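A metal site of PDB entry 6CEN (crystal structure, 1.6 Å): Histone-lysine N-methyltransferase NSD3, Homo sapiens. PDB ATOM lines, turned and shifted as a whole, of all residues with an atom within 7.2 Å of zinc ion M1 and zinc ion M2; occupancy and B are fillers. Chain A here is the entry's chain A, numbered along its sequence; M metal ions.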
ATOM      1  N   ARG A  40      16.054   8.303  -2.963  1.00  0.00           N
ATOM      2  CA  ARG A  40      16.510   7.240  -3.830  1.00  0.00           C
ATOM      3  C   ARG A  40      17.480   6.357  -3.068  1.00  0.00           C
ATOM      4  O   ARG A  40      18.423   6.843  -2.479  1.00  0.00           O
ATOM      5  CB  ARG A  40      17.216   7.836  -5.038  1.00  0.00           C
ATOM      6  CG  ARG A  40      17.634   6.820  -6.082  1.00  0.00           C
ATOM      7  CD  ARG A  40      18.653   7.387  -7.069  1.00  0.00           C
ATOM      8  NE  ARG A  40      18.012   8.326  -7.991  1.00  0.00           N
ATOM      9  CZ  ARG A  40      17.927   9.648  -7.841  1.00  0.00           C
ATOM     10  NH1 ARG A  40      18.440  10.284  -6.773  1.00  0.00           N
ATOM     11  NH2 ARG A  40      17.308  10.373  -8.775  1.00  0.00           N
ATOM     12  N   CYS A  41      17.233   5.044  -3.077  1.00  0.00           N
ATOM     13  CA  CYS A  41      18.131   4.088  -2.461  1.00  0.00           C
ATOM     14  C   CYS A  41      19.295   3.739  -3.408  1.00  0.00           C
ATOM     15  O   CYS A  41      19.318   4.182  -4.564  1.00  0.00           O
ATOM     16  CB  CYS A  41      17.362   2.834  -2.079  1.00  0.00           C
ATOM     17  SG  CYS A  41      16.883   1.754  -3.444  1.00  0.00           S
ATOM     18  N   ASN A  42      20.228   2.932  -2.908  1.00  0.00           N
ATOM     19  CA  ASN A  42      21.394   2.501  -3.682  1.00  0.00           C
ATOM     20  C   ASN A  42      21.342   1.040  -4.155  1.00  0.00           C
ATOM     21  O   ASN A  42      22.362   0.497  -4.588  1.00  0.00           O
ATOM     22  CB  ASN A  42      22.663   2.737  -2.869  1.00  0.00           C
ATOM     23  CG  ASN A  42      22.993   4.211  -2.713  1.00  0.00           C
ATOM     24  OD1 ASN A  42      22.710   5.024  -3.593  1.00  0.00           O
ATOM     25  ND2 ASN A  42      23.598   4.554  -1.594  1.00  0.00           N
ATOM     26  N   CYS A  43      20.157   0.407  -4.094  1.00  0.00           N
ATOM     27  CA  CYS A  43      20.005  -0.964  -4.566  1.00  0.00           C
ATOM     28  C   CYS A  43      20.182  -0.970  -6.078  1.00  0.00           C
ATOM     29  O   CYS A  43      19.999   0.062  -6.742  1.00  0.00           O
ATOM     30  CB  CYS A  43      18.633  -1.562  -4.200  1.00  0.00           C
ATOM     31  SG  CYS A  43      18.232  -1.637  -2.428  1.00  0.00           S
ATOM     32  N   LYS A  44      20.559  -2.121  -6.616  1.00  0.00           N
ATOM     33  CA  LYS A  44      20.803  -2.286  -8.059  1.00  0.00           C
ATOM     34  C   LYS A  44      19.692  -3.120  -8.704  1.00  0.00           C
ATOM     35  O   LYS A  44      19.246  -4.099  -8.125  1.00  0.00           O
ATOM     36  CB  LYS A  44      22.174  -2.928  -8.300  1.00  0.00           C
ATOM     37  CG  LYS A  44      23.291  -1.902  -8.406  1.00  0.00           C
ATOM     38  CD  LYS A  44      24.664  -2.546  -8.430  1.00  0.00           C
ATOM     39  CE  LYS A  44      25.708  -1.570  -8.939  1.00  0.00           C
ATOM     40  NZ  LYS A  44      27.107  -2.047  -8.703  1.00  0.00           N
ATOM     41  N   ASP A  47      19.989  -6.876  -8.672  1.00  0.00           N
ATOM     42  CA  ASP A  47      19.926  -7.589  -7.378  1.00  0.00           C
ATOM     43  C   ASP A  47      18.877  -8.680  -7.331  1.00  0.00           C
ATOM     44  O   ASP A  47      17.846  -8.576  -7.986  1.00  0.00           O
ATOM     45  CB  ASP A  47      19.613  -6.617  -6.219  1.00  0.00           C
ATOM     46  CG  ASP A  47      20.774  -5.684  -5.888  1.00  0.00           C
ATOM     47  OD1 ASP A  47      21.902  -5.899  -6.376  1.00  0.00           O
ATOM     48  OD2 ASP A  47      20.546  -4.717  -5.117  1.00  0.00           O
ATOM     49  N   PRO A  50      15.470  -6.909  -5.032  1.00  0.00           N
ATOM     50  CA  PRO A  50      15.884  -5.528  -4.824  1.00  0.00           C
ATOM     51  C   PRO A  50      14.908  -4.824  -3.881  1.00  0.00           C
ATOM     52  O   PRO A  50      13.700  -4.936  -4.053  1.00  0.00           O
ATOM     53  CB  PRO A  50      15.854  -4.918  -6.229  1.00  0.00           C
ATOM     54  CG  PRO A  50      14.986  -5.816  -7.033  1.00  0.00           C
ATOM     55  CD  PRO A  50      15.034  -7.164  -6.413  1.00  0.00           C
ATOM     56  N   CYS A  51      15.471  -4.133  -2.895  1.00  0.00           N
ATOM     57  CA  CYS A  51      14.710  -3.435  -1.866  1.00  0.00           C
ATOM     58  C   CYS A  51      13.847  -4.356  -0.990  1.00  0.00           C
ATOM     59  O   CYS A  51      12.881  -3.894  -0.376  1.00  0.00           O
ATOM     60  CB  CYS A  51      13.854  -2.331  -2.480  1.00  0.00           C
ATOM     61  SG  CYS A  51      14.797  -1.272  -3.606  1.00  0.00           S
ATOM     62  N   GLY A  52      14.225  -5.627  -0.902  1.00  0.00           N
ATOM     63  CA  GLY A  52      13.445  -6.617  -0.142  1.00  0.00           C
ATOM     64  C   GLY A  52      13.780  -6.632   1.340  1.00  0.00           C
ATOM     65  O   GLY A  52      14.664  -5.921   1.797  1.00  0.00           O
ATOM     66  N   SER A  55      17.349  -7.129   2.219  1.00  0.00           N
ATOM     67  CA  SER A  55      18.284  -6.263   1.497  1.00  0.00           C
ATOM     68  C   SER A  55      18.916  -5.254   2.414  1.00  0.00           C
ATOM     69  O   SER A  55      18.508  -5.067   3.567  1.00  0.00           O
ATOM     70  CB  SER A  55      17.561  -5.536   0.348  1.00  0.00           C
ATOM     71  OG  SER A  55      16.669  -4.546   0.829  1.00  0.00           O
ATOM     72  N   GLU A  56      19.922  -4.569   1.879  1.00  0.00           N
ATOM     73  CA  GLU A  56      20.550  -3.453   2.570  1.00  0.00           C
ATOM     74  C   GLU A  56      19.764  -2.134   2.408  1.00  0.00           C
ATOM     75  O   GLU A  56      20.269  -1.082   2.812  1.00  0.00           O
ATOM     76  CB  GLU A  56      22.012  -3.280   2.067  1.00  0.00           C
ATOM     77  CG  GLU A  56      22.219  -2.579   0.711  1.00  0.00           C
ATOM     78  CD  GLU A  56      21.762  -3.369  -0.510  1.00  0.00           C
ATOM     79  OE1 GLU A  56      21.399  -4.565  -0.371  1.00  0.00           O
ATOM     80  OE2 GLU A  56      21.773  -2.800  -1.631  1.00  0.00           O
ATOM     81  N   CYS A  57      18.551  -2.183   1.845  1.00  0.00           N
ATOM     82  CA  CYS A  57      17.932  -1.009   1.229  1.00  0.00           C
ATOM     83  C   CYS A  57      17.880   0.178   2.159  1.00  0.00           C
ATOM     84  O   CYS A  57      17.296   0.077   3.244  1.00  0.00           O
ATOM     85  CB  CYS A  57      16.495  -1.319   0.790  1.00  0.00           C
ATOM     86  SG  CYS A  57      15.735   0.057  -0.069  1.00  0.00           S
ATOM     87  N   LEU A  58      18.495   1.285   1.749  1.00  0.00           N
ATOM     88  CA  LEU A  58      18.545   2.508   2.578  1.00  0.00           C
ATOM     89  C   LEU A  58      17.142   3.062   2.856  1.00  0.00           C
ATOM     90  O   LEU A  58      16.892   3.574   3.944  1.00  0.00           O
ATOM     91  CB  LEU A  58      19.396   3.599   1.927  1.00  0.00           C
ATOM     92  CG  LEU A  58      20.910   3.453   1.962  1.00  0.00           C
ATOM     93  CD1 LEU A  58      21.548   4.571   1.136  1.00  0.00           C
ATOM     94  CD2 LEU A  58      21.424   3.472   3.390  1.00  0.00           C
ATOM     95  N   ASN A  59      16.256   2.992   1.872  1.00  0.00           N
ATOM     96  CA  ASN A  59      14.861   3.454   2.066  1.00  0.00           C
ATOM     97  C   ASN A  59      14.130   2.575   3.093  1.00  0.00           C
ATOM     98  O   ASN A  59      13.597   3.079   4.088  1.00  0.00           O
ATOM     99  CB  ASN A  59      14.094   3.498   0.728  1.00  0.00           C
ATOM    100  CG  ASN A  59      14.393   4.752  -0.084  1.00  0.00           C
ATOM    101  OD1 ASN A  59      15.134   5.638   0.345  1.00  0.00           O
ATOM    102  ND2 ASN A  59      13.754   4.874  -1.253  1.00  0.00           N
ATOM    103  N   ARG A  60      14.183   1.271   2.921  1.00  0.00           N
ATOM    104  CA  ARG A  60      13.448   0.345   3.768  1.00  0.00           C
ATOM    105  C   ARG A  60      13.994   0.423   5.195  1.00  0.00           C
ATOM    106  O   ARG A  60      13.215   0.427   6.158  1.00  0.00           O
ATOM    107  CB  ARG A  60      13.560  -1.079   3.207  1.00  0.00           C
ATOM    108  CG  ARG A  60      12.931  -2.179   4.021  1.00  0.00           C
ATOM    109  CD  ARG A  60      13.112  -3.521   3.328  1.00  0.00           C
ATOM    110  NE  ARG A  60      12.120  -3.752   2.285  1.00  0.00           N
ATOM    111  CZ  ARG A  60      10.841  -4.099   2.495  1.00  0.00           C
ATOM    112  NH1 ARG A  60      10.348  -4.216   3.729  1.00  0.00           N
ATOM    113  NH2 ARG A  60      10.045  -4.300   1.456  1.00  0.00           N
ATOM    114  N   GLU A  65       9.072   4.202   1.779  1.00  0.00           N
ATOM    115  CA  GLU A  65       8.661   3.408   0.622  1.00  0.00           C
ATOM    116  C   GLU A  65       9.303   3.981  -0.623  1.00  0.00           C
ATOM    117  O   GLU A  65       9.341   5.186  -0.809  1.00  0.00           O
ATOM    118  CB  GLU A  65       7.127   3.455   0.510  1.00  0.00           C
ATOM    119  CG  GLU A  65       6.597   2.866  -0.799  1.00  0.00           C
ATOM    120  CD  GLU A  65       5.351   2.030  -0.654  1.00  0.00           C
ATOM    121  OE1 GLU A  65       5.256   1.279   0.318  1.00  0.00           O
ATOM    122  OE2 GLU A  65       4.505   2.079  -1.550  1.00  0.00           O
ATOM    123  N   CYS A  66       9.800   3.103  -1.495  1.00  0.00           N
ATOM    124  CA  CYS A  66      10.308   3.536  -2.805  1.00  0.00           C
ATOM    125  C   CYS A  66       9.193   3.992  -3.729  1.00  0.00           C
ATOM    126  O   CYS A  66       8.072   3.500  -3.645  1.00  0.00           O
ATOM    127  CB  CYS A  66      11.032   2.371  -3.493  1.00  0.00           C
ATOM    128  SG  CYS A  66      12.581   1.904  -2.753  1.00  0.00           S
ATOM    129  N   HIS A  67       9.521   4.930  -4.618  1.00  0.00           N
ATOM    130  CA  HIS A  67       8.617   5.329  -5.704  1.00  0.00           C
ATOM    131  C   HIS A  67       9.253   4.750  -6.986  1.00  0.00           C
ATOM    132  O   HIS A  67      10.441   4.961  -7.233  1.00  0.00           O
ATOM    133  CB  HIS A  67       8.545   6.854  -5.744  1.00  0.00           C
ATOM    134  CG  HIS A  67       7.468   7.417  -6.626  1.00  0.00           C
ATOM    135  ND1 HIS A  67       7.472   7.279  -7.992  1.00  0.00           N
ATOM    136  CD2 HIS A  67       6.375   8.140  -6.332  1.00  0.00           C
ATOM    137  CE1 HIS A  67       6.429   7.893  -8.507  1.00  0.00           C
ATOM    138  NE2 HIS A  67       5.746   8.429  -7.520  1.00  0.00           N
ATOM    139  N   PRO A  68       8.481   4.002  -7.781  1.00  0.00           N
ATOM    140  CA  PRO A  68       9.055   3.231  -8.908  1.00  0.00           C
ATOM    141  C   PRO A  68       9.764   4.087  -9.986  1.00  0.00           C
ATOM    142  O   PRO A  68      10.754   3.648 -10.573  1.00  0.00           O
ATOM    143  CB  PRO A  68       7.824   2.508  -9.486  1.00  0.00           C
ATOM    144  CG  PRO A  68       6.668   3.312  -9.070  1.00  0.00           C
ATOM    145  CD  PRO A  68       7.017   3.904  -7.738  1.00  0.00           C
ATOM    146  N   VAL A  70      11.541   6.540  -9.228  1.00  0.00           N
ATOM    147  CA  VAL A  70      12.752   7.010  -8.567  1.00  0.00           C
ATOM    148  C   VAL A  70      13.758   5.895  -8.293  1.00  0.00           C
ATOM    149  O   VAL A  70      14.963   6.094  -8.421  1.00  0.00           O
ATOM    150  CB  VAL A  70      12.381   7.726  -7.234  1.00  0.00           C
ATOM    151  CG1 VAL A  70      13.616   8.221  -6.482  1.00  0.00           C
ATOM    152  CG2 VAL A  70      11.444   8.887  -7.520  1.00  0.00           C
ATOM    153  N   CYS A  71      13.273   4.727  -7.865  1.00  0.00           N
ATOM    154  CA  CYS A  71      14.155   3.665  -7.379  1.00  0.00           C
ATOM    155  C   CYS A  71      15.058   3.101  -8.494  1.00  0.00           C
ATOM    156  O   CYS A  71      14.569   2.850  -9.571  1.00  0.00           O
ATOM    157  CB  CYS A  71      13.293   2.542  -6.803  1.00  0.00           C
ATOM    158  SG  CYS A  71      14.202   1.117  -6.203  1.00  0.00           S
ATOM    159  N   PRO A  72      16.368   2.883  -8.236  1.00  0.00           N
ATOM    160  CA  PRO A  72      17.178   2.279  -9.312  1.00  0.00           C
ATOM    161  C   PRO A  72      16.684   0.914  -9.802  1.00  0.00           C
ATOM    162  O   PRO A  72      17.011   0.552 -10.931  1.00  0.00           O
ATOM    163  CB  PRO A  72      18.562   2.151  -8.666  1.00  0.00           C
ATOM    164  CG  PRO A  72      18.607   3.276  -7.700  1.00  0.00           C
ATOM    165  CD  PRO A  72      17.213   3.318  -7.118  1.00  0.00           C
ATOM    166  N   ALA A  73      15.920   0.195  -8.976  1.00  0.00           N
ATOM    167  CA  ALA A  73      15.397  -1.136  -9.312  1.00  0.00           C
ATOM    168  C   ALA A  73      14.179  -1.150 -10.230  1.00  0.00           C
ATOM    169  O   ALA A  73      13.761  -2.226 -10.634  1.00  0.00           O
ATOM    170  CB  ALA A  73      15.071  -1.925  -8.034  1.00  0.00           C
ATOM    171  N   GLY A  74      13.599   0.009 -10.549  1.00  0.00           N
ATOM    172  CA  GLY A  74      12.402   0.017 -11.392  1.00  0.00           C
ATOM    173  C   GLY A  74      11.207  -0.648 -10.728  1.00  0.00           C
ATOM    174  O   GLY A  74      11.004  -0.548  -9.513  1.00  0.00           O
ATOM    175  N   ARG A  76      10.880  -3.851 -10.433  1.00  0.00           N
ATOM    176  CA  ARG A  76      11.330  -5.015  -9.643  1.00  0.00           C
ATOM    177  C   ARG A  76      11.400  -4.714  -8.133  1.00  0.00           C
ATOM    178  O   ARG A  76      11.475  -5.639  -7.320  1.00  0.00           O
ATOM    179  CB  ARG A  76      12.718  -5.470 -10.106  1.00  0.00           C
ATOM    180  CG  ARG A  76      12.755  -6.067 -11.507  1.00  0.00           C
ATOM    181  CD  ARG A  76      14.052  -6.839 -11.747  1.00  0.00           C
ATOM    182  NE  ARG A  76      14.189  -8.017 -10.880  1.00  0.00           N
ATOM    183  CZ  ARG A  76      15.215  -8.288 -10.062  1.00  0.00           C
ATOM    184  NH1 ARG A  76      16.283  -7.489  -9.961  1.00  0.00           N
ATOM    185  NH2 ARG A  76      15.184  -9.404  -9.338  1.00  0.00           N
ATOM    186  N   CYS A  77      11.409  -3.425  -7.778  1.00  0.00           N
ATOM    187  CA  CYS A  77      11.493  -2.986  -6.392  1.00  0.00           C
ATOM    188  C   CYS A  77      10.467  -3.690  -5.494  1.00  0.00           C
ATOM    189  O   CYS A  77       9.273  -3.656  -5.784  1.00  0.00           O
ATOM    190  CB  CYS A  77      11.317  -1.470  -6.343  1.00  0.00           C
ATOM    191  SG  CYS A  77      11.203  -0.792  -4.662  1.00  0.00           S
ATOM    192  N   GLN A  78      10.936  -4.320  -4.418  1.00  0.00           N
ATOM    193  CA  GLN A  78      10.079  -4.988  -3.441  1.00  0.00           C
ATOM    194  C   GLN A  78       9.701  -4.105  -2.226  1.00  0.00           C
ATOM    195  O   GLN A  78       9.290  -4.599  -1.187  1.00  0.00           O
ATOM    196  CB  GLN A  78      10.754  -6.287  -2.948  1.00  0.00           C
ATOM    197  CG  GLN A  78      11.169  -7.181  -4.107  1.00  0.00           C
ATOM    198  CD  GLN A  78      11.588  -8.581  -3.693  1.00  0.00           C
ATOM    199  OE1 GLN A  78      11.808  -8.860  -2.523  1.00  0.00           O
ATOM    200  NE2 GLN A  78      11.714  -9.464  -4.684  1.00  0.00           N
ATOM    201  N   ASN A  79       9.876  -2.796  -2.365  1.00  0.00           N
ATOM    202  CA  ASN A  79       9.529  -1.829  -1.319  1.00  0.00           C
ATOM    203  C   ASN A  79       8.460  -0.839  -1.813  1.00  0.00           C
ATOM    204  O   ASN A  79       8.627   0.381  -1.696  1.00  0.00           O
ATOM    205  CB  ASN A  79      10.792  -1.100  -0.910  1.00  0.00           C
ATOM    206  CG  ASN A  79      10.609  -0.218   0.303  1.00  0.00           C
ATOM    207  OD1 ASN A  79       9.808  -0.511   1.183  1.00  0.00           O
ATOM    208  ND2 ASN A  79      11.362   0.847   0.361  1.00  0.00           N
ATOM    209  N   GLN A  80       7.370  -1.386  -2.354  1.00  0.00           N
ATOM    210  CA  GLN A  80       6.225  -0.625  -2.850  1.00  0.00           C
ATOM    211  C   GLN A  80       4.930  -1.142  -2.216  1.00  0.00           C
ATOM    212  O   GLN A  80       3.864  -1.081  -2.813  1.00  0.00           O
ATOM    213  CB  GLN A  80       6.122  -0.722  -4.372  1.00  0.00           C
ATOM    214  CG  GLN A  80       7.399  -0.361  -5.126  1.00  0.00           C
ATOM    215  CD  GLN A  80       7.209  -0.503  -6.621  1.00  0.00           C
ATOM    216  OE1 GLN A  80       6.426   0.230  -7.213  1.00  0.00           O
ATOM    217  NE2 GLN A  80       7.857  -1.504  -7.226  1.00  0.00           N
HETATM  218 ZN    ZN M   1      16.373  -0.202  -2.303  1.00  0.00          ZN
HETATM  219 ZN    ZN M   2      13.209   0.294  -4.301  1.00  0.00          ZN
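Zinc ion M1 is bound by the side-chain sulfur (SG) of Cys 51 (2.3 Å), the side-chain sulfur (SG) of Cys 41 (2.3 Å), the side-chain sulfur (SG) of Cys 57 (2.3 Å) and the side-chain sulfur (SG) of Cys 43 (2.4 Å).
SG of Cys 77 lies close to N of Asn 79, 3.3 Å away. O of Cys 51 lies within hydrogen-bond range of NE of Arg 60, 2.8 Å away. N of Ala 73 lies close to SG of Cys 71 (3.4 Å). The backbone NH (N) of Cys 66 sits at hydrogen-bond distance from the backbone carbonyl oxygen (O) of Asn 79 (3.0 Å). NE2 of Gln 80 sits at hydrogen-bond distance from O of Cys 77, at 3.0 Å. N of Arg 60 sits close to SG of Cys 57 (3.6 Å). The side-chain sulfur (SG) of Cys 57 lies close to the backbone NH (N) of Asn 59, at 3.6 Å. N of Cys 57 sits close to OG of Ser 55, at 3.2 Å.
Four residues have an atom within 4 Å of zinc ion M2: Cys 51, Cys 66, Cys 71 and Cys 77. Along chain A the residues within 4 Å of zinc ion M2 span positions 51 to 77.
Zinc ion M2 is bound by the side-chain sulfur of Cys 71 (2.3 Å), the side-chain sulfur of Cys 77 (2.3 Å), the side-chain sulfur of Cys 66 (2.3 Å) and the side-chain sulfur of Cys 51 (2.3 Å).
Of the 29 residues printed, 4 come within 4 Å of zinc ion M1. The nearest printed residue that does not touch zinc ion M1 is Cys 66 (4.4 Å).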
